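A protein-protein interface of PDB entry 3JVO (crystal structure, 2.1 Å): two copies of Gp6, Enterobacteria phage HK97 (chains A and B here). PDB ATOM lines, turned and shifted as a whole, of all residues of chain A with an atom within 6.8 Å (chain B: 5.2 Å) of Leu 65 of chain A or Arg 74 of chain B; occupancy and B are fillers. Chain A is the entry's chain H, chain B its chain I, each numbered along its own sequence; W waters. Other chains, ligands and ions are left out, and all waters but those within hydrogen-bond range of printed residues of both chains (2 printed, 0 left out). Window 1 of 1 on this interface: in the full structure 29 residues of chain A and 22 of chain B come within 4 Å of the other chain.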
ATOM      1  N   LYS A  15       4.543   2.598 -14.675  1.00  0.00           N
ATOM      2  CA  LYS A  15       4.988   1.366 -14.021  1.00  0.00           C
ATOM      3  C   LYS A  15       4.503   0.139 -14.756  1.00  0.00           C
ATOM      4  O   LYS A  15       5.192  -0.875 -14.752  1.00  0.00           O
ATOM      5  CB  LYS A  15       4.520   1.310 -12.568  1.00  0.00           C
ATOM      6  CG  LYS A  15       5.162   2.378 -11.660  1.00  0.00           C
ATOM      7  CD  LYS A  15       4.745   2.051 -10.224  1.00  0.00           C
ATOM      8  CE  LYS A  15       4.823   3.222  -9.328  1.00  0.00           C
ATOM      9  NZ  LYS A  15       4.228   2.819  -7.979  1.00  0.00           N
ATOM     10  N   GLN A  16       3.305   0.213 -15.345  1.00  0.00           N
ATOM     11  CA  GLN A  16       2.783  -0.919 -16.126  1.00  0.00           C
ATOM     12  C   GLN A  16       3.617  -1.171 -17.376  1.00  0.00           C
ATOM     13  O   GLN A  16       3.839  -2.314 -17.723  1.00  0.00           O
ATOM     14  CB  GLN A  16       1.312  -0.712 -16.502  1.00  0.00           C
ATOM     15  CG  GLN A  16       0.345  -0.916 -15.331  1.00  0.00           C
ATOM     16  CD  GLN A  16      -1.096  -0.763 -15.741  1.00  0.00           C
ATOM     17  OE1 GLN A  16      -1.454  -0.837 -16.928  1.00  0.00           O
ATOM     18  NE2 GLN A  16      -1.949  -0.540 -14.761  1.00  0.00           N
ATOM     19  N   GLN A  17       4.042  -0.094 -18.049  1.00  0.00           N
ATOM     20  CA  GLN A  17       4.937  -0.147 -19.220  1.00  0.00           C
ATOM     21  C   GLN A  17       6.182  -0.990 -18.961  1.00  0.00           C
ATOM     22  O   GLN A  17       6.618  -1.769 -19.807  1.00  0.00           O
ATOM     23  CB  GLN A  17       5.382   1.282 -19.615  1.00  0.00           C
ATOM     24  CG  GLN A  17       6.399   1.360 -20.802  1.00  0.00           C
ATOM     25  CD  GLN A  17       5.783   0.931 -22.139  1.00  0.00           C
ATOM     26  OE1 GLN A  17       4.593   0.624 -22.207  1.00  0.00           O
ATOM     27  NE2 GLN A  17       6.593   0.935 -23.220  1.00  0.00           N
ATOM     28  N   ILE A  18       6.776  -0.822 -17.787  1.00  0.00           N
ATOM     29  CA  ILE A  18       7.991  -1.531 -17.468  1.00  0.00           C
ATOM     30  C   ILE A  18       7.696  -2.721 -16.537  1.00  0.00           C
ATOM     31  O   ILE A  18       8.624  -3.326 -15.976  1.00  0.00           O
ATOM     32  CB  ILE A  18       9.010  -0.597 -16.778  1.00  0.00           C
ATOM     33  CG1 ILE A  18       8.335   0.217 -15.671  1.00  0.00           C
ATOM     34  CG2 ILE A  18       9.703   0.328 -17.793  1.00  0.00           C
ATOM     35  CD1 ILE A  18       9.360   0.841 -14.738  1.00  0.00           C
ATOM     36  N   GLU A  19       6.417  -3.065 -16.376  1.00  0.00           N
ATOM     37  CA  GLU A  19       6.025  -4.224 -15.545  1.00  0.00           C
ATOM     38  C   GLU A  19       6.659  -4.176 -14.141  1.00  0.00           C
ATOM     39  O   GLU A  19       7.260  -5.138 -13.705  1.00  0.00           O
ATOM     40  CB  GLU A  19       6.385  -5.550 -16.254  1.00  0.00           C
ATOM     41  CG  GLU A  19       5.615  -5.812 -17.563  1.00  0.00           C
ATOM     42  CD  GLU A  19       4.098  -5.799 -17.359  1.00  0.00           C
ATOM     43  OE1 GLU A  19       3.641  -6.244 -16.274  1.00  0.00           O
ATOM     44  OE2 GLU A  19       3.355  -5.338 -18.269  1.00  0.00           O
ATOM     45  N   ALA A  36      11.922  11.547 -20.524  1.00  0.00           N
ATOM     46  CA  ALA A  36      11.313  11.066 -21.775  1.00  0.00           C
ATOM     47  C   ALA A  36      10.368  12.106 -22.404  1.00  0.00           C
ATOM     48  O   ALA A  36      10.418  12.387 -23.605  1.00  0.00           O
ATOM     49  CB  ALA A  36      10.574   9.777 -21.529  1.00  0.00           C
ATOM     50  N   LYS A  60       2.271  10.093 -26.954  1.00  0.00           N
ATOM     51  CA  LYS A  60       2.244   9.381 -25.697  1.00  0.00           C
ATOM     52  C   LYS A  60       2.900   8.011 -25.832  1.00  0.00           C
ATOM     53  O   LYS A  60       3.690   7.618 -24.985  1.00  0.00           O
ATOM     54  CB  LYS A  60       0.805   9.292 -25.200  1.00  0.00           C
ATOM     55  CG  LYS A  60       0.326  10.633 -24.652  1.00  0.00           C
ATOM     56  CD  LYS A  60      -1.150  10.719 -24.466  1.00  0.00           C
ATOM     57  CE  LYS A  60      -1.540  10.063 -23.174  1.00  0.00           C
ATOM     58  NZ  LYS A  60      -3.028  10.032 -23.011  1.00  0.00           N
ATOM     59  N   GLY A  61       2.621   7.302 -26.928  1.00  0.00           N
ATOM     60  CA  GLY A  61       3.283   6.017 -27.179  1.00  0.00           C
ATOM     61  C   GLY A  61       4.805   6.143 -27.288  1.00  0.00           C
ATOM     62  O   GLY A  61       5.545   5.312 -26.735  1.00  0.00           O
ATOM     63  N   ALA A  62       5.277   7.175 -27.980  1.00  0.00           N
ATOM     64  CA  ALA A  62       6.723   7.422 -28.104  1.00  0.00           C
ATOM     65  C   ALA A  62       7.312   7.743 -26.730  1.00  0.00           C
ATOM     66  O   ALA A  62       8.410   7.292 -26.409  1.00  0.00           O
ATOM     67  CB  ALA A  62       7.004   8.559 -29.082  1.00  0.00           C
ATOM     68  N   VAL A  63       6.574   8.496 -25.909  1.00  0.00           N
ATOM     69  CA  VAL A  63       7.066   8.809 -24.574  1.00  0.00           C
ATOM     70  C   VAL A  63       7.273   7.513 -23.794  1.00  0.00           C
ATOM     71  O   VAL A  63       8.309   7.345 -23.144  1.00  0.00           O
ATOM     72  CB  VAL A  63       6.142   9.778 -23.806  1.00  0.00           C
ATOM     73  CG1 VAL A  63       6.586   9.934 -22.343  1.00  0.00           C
ATOM     74  CG2 VAL A  63       6.171  11.138 -24.475  1.00  0.00           C
ATOM     75  N   LEU A  64       6.309   6.590 -23.867  1.00  0.00           N
ATOM     76  CA  LEU A  64       6.434   5.319 -23.130  1.00  0.00           C
ATOM     77  C   LEU A  64       7.647   4.505 -23.592  1.00  0.00           C
ATOM     78  O   LEU A  64       8.289   3.825 -22.771  1.00  0.00           O
ATOM     79  CB  LEU A  64       5.188   4.453 -23.305  1.00  0.00           C
ATOM     80  CG  LEU A  64       3.917   4.869 -22.552  1.00  0.00           C
ATOM     81  CD1 LEU A  64       2.776   3.921 -22.941  1.00  0.00           C
ATOM     82  CD2 LEU A  64       4.160   4.894 -21.021  1.00  0.00           C
ATOM     83  N   LEU A  65       7.935   4.534 -24.896  1.00  0.00           N
ATOM     84  CA  LEU A  65       9.089   3.809 -25.466  1.00  0.00           C
ATOM     85  C   LEU A  65      10.411   4.419 -24.980  1.00  0.00           C
ATOM     86  O   LEU A  65      11.328   3.695 -24.617  1.00  0.00           O
ATOM     87  CB  LEU A  65       9.046   3.841 -26.994  1.00  0.00           C
ATOM     88  CG  LEU A  65       7.924   3.022 -27.673  1.00  0.00           C
ATOM     89  CD1 LEU A  65       7.829   3.328 -29.161  1.00  0.00           C
ATOM     90  CD2 LEU A  65       8.158   1.540 -27.472  1.00  0.00           C
ATOM     91  N   VAL A  66      10.505   5.751 -24.996  1.00  0.00           N
ATOM     92  CA  VAL A  66      11.727   6.439 -24.564  1.00  0.00           C
ATOM     93  C   VAL A  66      11.940   6.203 -23.063  1.00  0.00           C
ATOM     94  O   VAL A  66      13.050   5.927 -22.615  1.00  0.00           O
ATOM     95  CB  VAL A  66      11.682   7.946 -24.919  1.00  0.00           C
ATOM     96  CG1 VAL A  66      12.890   8.718 -24.327  1.00  0.00           C
ATOM     97  CG2 VAL A  66      11.643   8.118 -26.468  1.00  0.00           C
ATOM     98  N   PHE A  67      10.845   6.284 -22.302  1.00  0.00           N
ATOM     99  CA  PHE A  67      10.896   6.086 -20.863  1.00  0.00           C
ATOM    100  C   PHE A  67      11.399   4.680 -20.494  1.00  0.00           C
ATOM    101  O   PHE A  67      12.284   4.515 -19.626  1.00  0.00           O
ATOM    102  CB  PHE A  67       9.494   6.300 -20.288  1.00  0.00           C
ATOM    103  CG  PHE A  67       9.272   5.597 -18.983  1.00  0.00           C
ATOM    104  CD1 PHE A  67       9.690   6.191 -17.767  1.00  0.00           C
ATOM    105  CD2 PHE A  67       8.633   4.349 -18.949  1.00  0.00           C
ATOM    106  CE1 PHE A  67       9.483   5.521 -16.546  1.00  0.00           C
ATOM    107  CE2 PHE A  67       8.434   3.687 -17.727  1.00  0.00           C
ATOM    108  CZ  PHE A  67       8.865   4.279 -16.539  1.00  0.00           C
ATOM    109  N   ALA A  68      10.806   3.679 -21.148  1.00  0.00           N
ATOM    110  CA  ALA A  68      11.114   2.268 -20.880  1.00  0.00           C
ATOM    111  C   ALA A  68      12.573   1.983 -21.231  1.00  0.00           C
ATOM    112  O   ALA A  68      13.264   1.269 -20.508  1.00  0.00           O
ATOM    113  CB  ALA A  68      10.192   1.357 -21.655  1.00  0.00           C
ATOM    114  N   ASP A  69      13.038   2.567 -22.332  1.00  0.00           N
ATOM    115  CA  ASP A  69      14.451   2.463 -22.693  1.00  0.00           C
ATOM    116  C   ASP A  69      15.395   2.956 -21.562  1.00  0.00           C
ATOM    117  O   ASP A  69      16.422   2.308 -21.299  1.00  0.00           O
ATOM    118  CB  ASP A  69      14.720   3.178 -24.009  1.00  0.00           C
ATOM    119  CG  ASP A  69      16.152   2.995 -24.489  1.00  0.00           C
ATOM    120  OD1 ASP A  69      16.602   1.834 -24.650  1.00  0.00           O
ATOM    121  OD2 ASP A  69      16.855   4.022 -24.679  1.00  0.00           O
ATOM    122  N   MET A  70      15.035   4.063 -20.882  1.00  0.00           N
ATOM    123  CA  MET A  70      15.812   4.621 -19.752  1.00  0.00           C
ATOM    124  C   MET A  70      15.802   3.698 -18.545  1.00  0.00           C
ATOM    125  O   MET A  70      16.776   3.602 -17.828  1.00  0.00           O
ATOM    126  CB  MET A  70      15.242   5.970 -19.282  1.00  0.00           C
ATOM    127  CG  MET A  70      15.332   7.125 -20.263  1.00  0.00           C
ATOM    128  SD  MET A  70      17.172   7.680 -20.634  1.00  0.00           S
ATOM    129  CE  MET A  70      17.860   8.066 -18.825  1.00  0.00           C
ATOM    130  N   ASN A  85      14.576   1.025 -32.115  1.00  0.00           N
ATOM    131  CA  ASN A  85      13.219   0.573 -32.414  1.00  0.00           C
ATOM    132  C   ASN A  85      12.578   1.719 -33.178  1.00  0.00           C
ATOM    133  O   ASN A  85      12.284   2.758 -32.590  1.00  0.00           O
ATOM    134  CB  ASN A  85      12.427   0.277 -31.120  1.00  0.00           C
ATOM    135  CG  ASN A  85      10.957  -0.045 -31.386  1.00  0.00           C
ATOM    136  OD1 ASN A  85      10.476   0.060 -32.513  1.00  0.00           O
ATOM    137  ND2 ASN A  85      10.248  -0.442 -30.358  1.00  0.00           N
ATOM    138  N   ALA A  86      12.360   1.511 -34.474  1.00  0.00           N
ATOM    139  CA  ALA A  86      11.832   2.521 -35.389  1.00  0.00           C
ATOM    140  C   ALA A  86      10.499   3.133 -34.958  1.00  0.00           C
ATOM    141  O   ALA A  86      10.178   4.265 -35.356  1.00  0.00           O
ATOM    142  CB  ALA A  86      11.683   1.926 -36.802  1.00  0.00           C
ATOM    143  N   ALA A  87       9.734   2.389 -34.167  1.00  0.00           N
ATOM    144  CA  ALA A  87       8.405   2.835 -33.711  1.00  0.00           C
ATOM    145  C   ALA A  87       8.439   4.182 -33.001  1.00  0.00           C
ATOM    146  O   ALA A  87       7.482   4.939 -33.112  1.00  0.00           O
ATOM    147  CB  ALA A  87       7.740   1.768 -32.800  1.00  0.00           C
ATOM    148  N   ALA A  88       9.529   4.488 -32.291  1.00  0.00           N
ATOM    149  CA  ALA A  88       9.600   5.741 -31.522  1.00  0.00           C
ATOM    150  C   ALA A  88       9.616   6.972 -32.429  1.00  0.00           C
ATOM    151  O   ALA A  88       8.740   7.836 -32.299  1.00  0.00           O
ATOM    152  CB  ALA A  88      10.786   5.746 -30.536  1.00  0.00           C
ATOM    153  N   GLU A  89      10.560   7.019 -33.378  1.00  0.00           N
ATOM    154  CA  GLU A  89      10.653   8.119 -34.329  1.00  0.00           C
ATOM    155  C   GLU A  89       9.369   8.234 -35.135  1.00  0.00           C
ATOM    156  O   GLU A  89       8.829   9.325 -35.280  1.00  0.00           O
ATOM    157  CB  GLU A  89      11.899   7.992 -35.245  1.00  0.00           C
ATOM    158  CG  GLU A  89      11.664   7.507 -36.711  1.00  0.00           C
ATOM    159  CD  GLU A  89      11.434   8.654 -37.741  1.00  0.00           C
ATOM    160  OE1 GLU A  89      12.037   9.757 -37.593  1.00  0.00           O
ATOM    161  OE2 GLU A  89      10.665   8.441 -38.722  1.00  0.00           O
ATOM    162  N   MET A  91       6.171   7.236 -34.525  1.00  0.00           N
ATOM    163  CA  MET A  91       5.071   7.804 -33.712  1.00  0.00           C
ATOM    164  C   MET A  91       5.177   9.330 -33.562  1.00  0.00           C
ATOM    165  O   MET A  91       4.183  10.030 -33.522  1.00  0.00           O
ATOM    166  CB  MET A  91       5.095   7.220 -32.312  1.00  0.00           C
ATOM    167  CG  MET A  91       4.760   5.762 -32.250  1.00  0.00           C
ATOM    168  SD  MET A  91       2.847   5.431 -32.246  1.00  0.00           S
ATOM    169  CE  MET A  91       3.068   4.215 -30.811  1.00  0.00           C
ATOM    170  N   LEU B  28      -3.147   0.633 -19.883  1.00  0.00           N
ATOM    171  CA  LEU B  28      -1.994   0.502 -20.769  1.00  0.00           C
ATOM    172  C   LEU B  28      -2.413   0.086 -22.187  1.00  0.00           C
ATOM    173  O   LEU B  28      -2.054   0.756 -23.193  1.00  0.00           O
ATOM    174  CB  LEU B  28      -0.980  -0.476 -20.181  1.00  0.00           C
ATOM    175  CG  LEU B  28       0.282  -0.568 -21.035  1.00  0.00           C
ATOM    176  CD1 LEU B  28       1.113   0.735 -20.912  1.00  0.00           C
ATOM    177  CD2 LEU B  28       1.099  -1.786 -20.668  1.00  0.00           C
ATOM    178  N   TYR B  32      -2.005   2.138 -25.867  1.00  0.00           N
ATOM    179  CA  TYR B  32      -1.409   1.532 -27.054  1.00  0.00           C
ATOM    180  C   TYR B  32      -2.387   1.551 -28.237  1.00  0.00           C
ATOM    181  O   TYR B  32      -2.011   1.832 -29.362  1.00  0.00           O
ATOM    182  CB  TYR B  32      -1.043   0.077 -26.798  1.00  0.00           C
ATOM    183  CG  TYR B  32       0.083  -0.207 -25.852  1.00  0.00           C
ATOM    184  CD1 TYR B  32       1.104   0.722 -25.601  1.00  0.00           C
ATOM    185  CD2 TYR B  32       0.140  -1.445 -25.208  1.00  0.00           C
ATOM    186  CE1 TYR B  32       2.155   0.416 -24.720  1.00  0.00           C
ATOM    187  CE2 TYR B  32       1.188  -1.770 -24.332  1.00  0.00           C
ATOM    188  CZ  TYR B  32       2.177  -0.837 -24.084  1.00  0.00           C
ATOM    189  OH  TYR B  32       3.193  -1.197 -23.227  1.00  0.00           O
ATOM    190  N   ASP B  69       2.660  -4.656 -31.692  1.00  0.00           N
ATOM    191  CA  ASP B  69       4.071  -4.274 -31.650  1.00  0.00           C
ATOM    192  C   ASP B  69       4.415  -3.431 -30.396  1.00  0.00           C
ATOM    193  O   ASP B  69       5.405  -3.697 -29.740  1.00  0.00           O
ATOM    194  CB  ASP B  69       4.461  -3.503 -32.918  1.00  0.00           C
ATOM    195  CG  ASP B  69       5.934  -3.186 -32.957  1.00  0.00           C
ATOM    196  OD1 ASP B  69       6.742  -4.139 -32.824  1.00  0.00           O
ATOM    197  OD2 ASP B  69       6.297  -1.988 -33.074  1.00  0.00           O
ATOM    198  N   MET B  70       3.603  -2.426 -30.078  1.00  0.00           N
ATOM    199  CA  MET B  70       3.767  -1.599 -28.861  1.00  0.00           C
ATOM    200  C   MET B  70       3.731  -2.448 -27.608  1.00  0.00           C
ATOM    201  O   MET B  70       4.484  -2.234 -26.661  1.00  0.00           O
ATOM    202  CB  MET B  70       2.628  -0.578 -28.723  1.00  0.00           C
ATOM    203  CG  MET B  70       2.538   0.452 -29.802  1.00  0.00           C
ATOM    204  SD  MET B  70       4.068   1.632 -29.741  1.00  0.00           S
ATOM    205  CE  MET B  70       4.094   2.141 -27.826  1.00  0.00           C
ATOM    206  N   PHE B  71       2.807  -3.391 -27.590  1.00  0.00           N
ATOM    207  CA  PHE B  71       2.651  -4.237 -26.415  1.00  0.00           C
ATOM    208  C   PHE B  71       3.850  -5.142 -26.233  1.00  0.00           C
ATOM    209  O   PHE B  71       4.241  -5.421 -25.114  1.00  0.00           O
ATOM    210  CB  PHE B  71       1.364  -5.076 -26.487  1.00  0.00           C
ATOM    211  CG  PHE B  71       1.104  -5.883 -25.242  1.00  0.00           C
ATOM    212  CD1 PHE B  71       0.430  -5.316 -24.163  1.00  0.00           C
ATOM    213  CD2 PHE B  71       1.541  -7.199 -25.146  1.00  0.00           C
ATOM    214  CE1 PHE B  71       0.207  -6.064 -22.993  1.00  0.00           C
ATOM    215  CE2 PHE B  71       1.330  -7.948 -24.003  1.00  0.00           C
ATOM    216  CZ  PHE B  71       0.668  -7.385 -22.922  1.00  0.00           C
ATOM    217  N   GLU B  72       4.422  -5.615 -27.334  1.00  0.00           N
ATOM    218  CA  GLU B  72       5.472  -6.624 -27.252  1.00  0.00           C
ATOM    219  C   GLU B  72       6.851  -6.018 -27.173  1.00  0.00           C
ATOM    220  O   GLU B  72       7.745  -6.623 -26.607  1.00  0.00           O
ATOM    221  CB  GLU B  72       5.415  -7.572 -28.439  1.00  0.00           C
ATOM    222  CG  GLU B  72       4.147  -8.409 -28.492  1.00  0.00           C
ATOM    223  CD  GLU B  72       4.005  -9.382 -27.318  1.00  0.00           C
ATOM    224  OE1 GLU B  72       5.012  -9.968 -26.854  1.00  0.00           O
ATOM    225  OE2 GLU B  72       2.856  -9.587 -26.873  1.00  0.00           O
ATOM    226  N   HIS B  73       7.021  -4.825 -27.749  1.00  0.00           N
ATOM    227  CA  HIS B  73       8.334  -4.225 -27.834  1.00  0.00           C
ATOM    228  C   HIS B  73       8.255  -2.845 -27.239  1.00  0.00           C
ATOM    229  O   HIS B  73       7.855  -1.869 -27.909  1.00  0.00           O
ATOM    230  CB  HIS B  73       8.816  -4.184 -29.279  1.00  0.00           C
ATOM    231  CG  HIS B  73       8.733  -5.504 -29.971  1.00  0.00           C
ATOM    232  ND1 HIS B  73       7.978  -5.704 -31.108  1.00  0.00           N
ATOM    233  CD2 HIS B  73       9.280  -6.709 -29.665  1.00  0.00           C
ATOM    234  CE1 HIS B  73       8.083  -6.968 -31.488  1.00  0.00           C
ATOM    235  NE2 HIS B  73       8.858  -7.600 -30.625  1.00  0.00           N
ATOM    236  N   ARG B  74       8.675  -2.785 -25.985  1.00  0.00           N
ATOM    237  CA  ARG B  74       8.356  -1.687 -25.084  1.00  0.00           C
ATOM    238  C   ARG B  74       9.429  -0.624 -24.978  1.00  0.00           C
ATOM    239  O   ARG B  74       9.188   0.398 -24.357  1.00  0.00           O
ATOM    240  CB  ARG B  74       8.056  -2.240 -23.694  1.00  0.00           C
ATOM    241  CG  ARG B  74       6.964  -3.302 -23.720  1.00  0.00           C
ATOM    242  CD  ARG B  74       5.982  -3.055 -22.662  1.00  0.00           C
ATOM    243  NE  ARG B  74       4.829  -3.923 -22.791  1.00  0.00           N
ATOM    244  CZ  ARG B  74       4.061  -4.230 -21.755  1.00  0.00           C
ATOM    245  NH1 ARG B  74       4.326  -3.712 -20.554  1.00  0.00           N
ATOM    246  NH2 ARG B  74       3.026  -5.037 -21.916  1.00  0.00           N
ATOM    247  N   THR B  75      10.600  -0.852 -25.579  1.00  0.00           N
ATOM    248  CA  THR B  75      11.706   0.099 -25.452  1.00  0.00           C
ATOM    249  C   THR B  75      12.083   0.748 -26.797  1.00  0.00           C
ATOM    250  O   THR B  75      11.999   0.095 -27.839  1.00  0.00           O
ATOM    251  CB  THR B  75      12.965  -0.579 -24.850  1.00  0.00           C
ATOM    252  OG1 THR B  75      13.256  -1.758 -25.601  1.00  0.00           O
ATOM    253  CG2 THR B  75      12.715  -0.992 -23.439  1.00  0.00           C
ATOM    254  N   ALA B  76      12.520   2.014 -26.756  1.00  0.00           N
ATOM    255  CA  ALA B  76      12.967   2.733 -27.965  1.00  0.00           C
ATOM    256  C   ALA B  76      14.240   2.152 -28.551  1.00  0.00           C
ATOM    257  O   ALA B  76      14.552   2.403 -29.721  1.00  0.00           O
ATOM    258  CB  ALA B  76      13.171   4.222 -27.690  1.00  0.00           C
HETATM  259  O   HOH W   1       7.572  -0.690 -30.483  1.00  0.00           O
HETATM  260  O   HOH W   2       5.532   0.094 -25.815  1.00  0.00           O
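The backbone carbonyl oxygen (O) of Gln 16 of chain A lies within hydrogen-bond range of the guanidinium group (NH1) of Arg 74 of chain B. The side-chain amide oxygen (OE1) of Gln 17 of chain A lies within hydrogen-bond range of the side-chain hydroxyl (OH) of Tyr 32 of chain B (2.5 Å). The backbone carbonyl oxygen (O) of Arg 74 of chain B is in hydrogen-bond range of the side-chain amide nitrogen (NE2) of Gln 17 of chain A, 2.9 Å away. NH1 of Arg 74 of chain B lies within salt-bridge range of OE2 of Glu 19 of chain A (3.0 Å). The backbone carbonyl oxygen of Leu 65 of chain A is in hydrogen-bond range of the backbone NH of Ala 76 of chain B, 3.0 Å away. ND2 of Asn 85 of chain A is in hydrogen-bond range of O of Thr 75 of chain B, at 3.1 Å. N of Asn 85 of chain A sits at hydrogen-bond distance from O of Ala 76 of chain B (2.8 Å).
The side-chain amide nitrogen of Gln 17 of chain A is in hydrogen-bond range of the backbone carbonyl oxygen of Leu 64 of chain A. N of Ala 87 of chain A sits at hydrogen-bond distance from OD1 of Asn 85 of chain A (3.0 Å). The side-chain hydroxyl (OH) of Tyr 32 of chain B lies within hydrogen-bond range of the guanidinium group (NE) of Arg 74 of chain B, at 3.2 Å. The side-chain carboxylate (OD1) of Asp 69 of chain B lies within hydrogen-bond range of a ring nitrogen (ND1) of His 73 of chain B. The backbone carbonyl oxygen (O) of Phe 71 of chain B is in hydrogen-bond range of the guanidinium group (NE) of Arg 74 of chain B, 2.8 Å away.
Gln 16 of chain A touches Leu 28 of chain B (OE1 to CB, 3.3 Å). Gln 17 of chain A touches Leu 28 of chain B (OE1 to CD1, 3.7 Å). CE of Met 70 of chain B touches CG of Leu 65 of chain A, at 3.9 Å. Thr 75 of chain B touches Leu 65 of chain A. Arg 74 of chain B touches Ala 68 of chain A. Thr 75 of chain B touches Ala 68 of chain A. CG2 of Thr 75 of chain B touches N of Asp 69 of chain A, 3.7 Å away. Asp 69 of chain A touches Ala 76 of chain B. Asn 85 of chain A touches His 73 of chain B. SD of Met 70 of chain B touches CE of Met 91 of chain A, 3.0 Å away.
Printed residues of chain B within 4 Å of Leu 65 of chain A: Met 70 (3.9 Å), His 73 (3.5 Å), Arg 74 (3.5 Å), Thr 75 (3.7 Å) and Ala 76 (3.0 Å). Of chain A, only Gln 16 (3.2 Å), Gln 17 (2.9 Å), Glu 19 (3.0 Å), Leu 64 (3.9 Å), Leu 65 (3.5 Å) and Ala 68 (3.0 Å) come within 4 Å of Arg 74 of chain B. Printed residues of chain B within 4 Å of Met 91 of chain A: Met 70. Printed residues of chain A within 4 Å of Tyr 32 of chain B: Gln 17 and Leu 64. Printed residues of chain A within 4 Å of His 73 of chain B: Leu 65 (3.5 Å) and Asn 85 (3.7 Å). Of the printed residues of chain A, Thr 75 of chain B touches Leu 65 (3.7 Å), Ala 68 (3.7 Å), Asp 69 (3.7 Å) and Asn 85 (3.1 Å). Met 70 of chain A touches none of the printed residues of chain B. The nearest printed residue of chain B that does not touch Leu 65 of chain A is Asp 69 of chain B (6.3 Å). The nearest printed residue of chain B that does not touch Ala 68 of chain A is Ala 76 of chain B (5.5 Å).
Printed residues of chain B that touch a printed residue of chain A: Leu 28, Tyr 32, Met 70, His 73, Arg 74, Thr 75 and Ala 76. Hydrophobic or aromatic side chains of chain B that line the printed part of chain A: Leu 28, Tyr 32, Met 70 and Ala 76. Of the 23 printed residues of chain A, 10 touch a printed residue of chain B. Printed residues of chain A that touch a printed residue of chain B: Gln 16, Gln 17, Glu 19, Gly 61, Leu 64, Leu 65, Ala 68, Asp 69, Asn 85 and Met 91. Hydrophobic or aromatic side chains of chain A within 4 Å of the printed part of chain B: Leu 64, Leu 65, Ala 68 and Met 91. Along chain A the printed residues that touch a printed residue of chain B span positions 16 to 91. Among the printed residues, Asp or Glu carboxylates within 4 Å of a Lys or Arg side-chain nitrogen of the other chain: Glu 19 of chain A with Arg 74 of chain B (3.0 Å).
Positions printed for both chains: 69 and 70. Of the 22 pairs that touch across the chains among the printed residues, none has its exchanged pair printed and touching as well.
Water W2 bridges the backbone carbonyl oxygen (O) of Met 70 of chain B (2.7 Å) and the side-chain amide nitrogen (NE2) of Gln 17 of chain A (2.9 Å). Water W1 lies within hydrogen-bond range of the side-chain amide nitrogen (ND2) of Asn 85 of chain A (2.7 Å), the backbone carbonyl oxygen (O) of His 73 of chain B (2.8 Å) and the side-chain carboxylate (OD2) of Asp 69 of chain B (3.2 Å).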
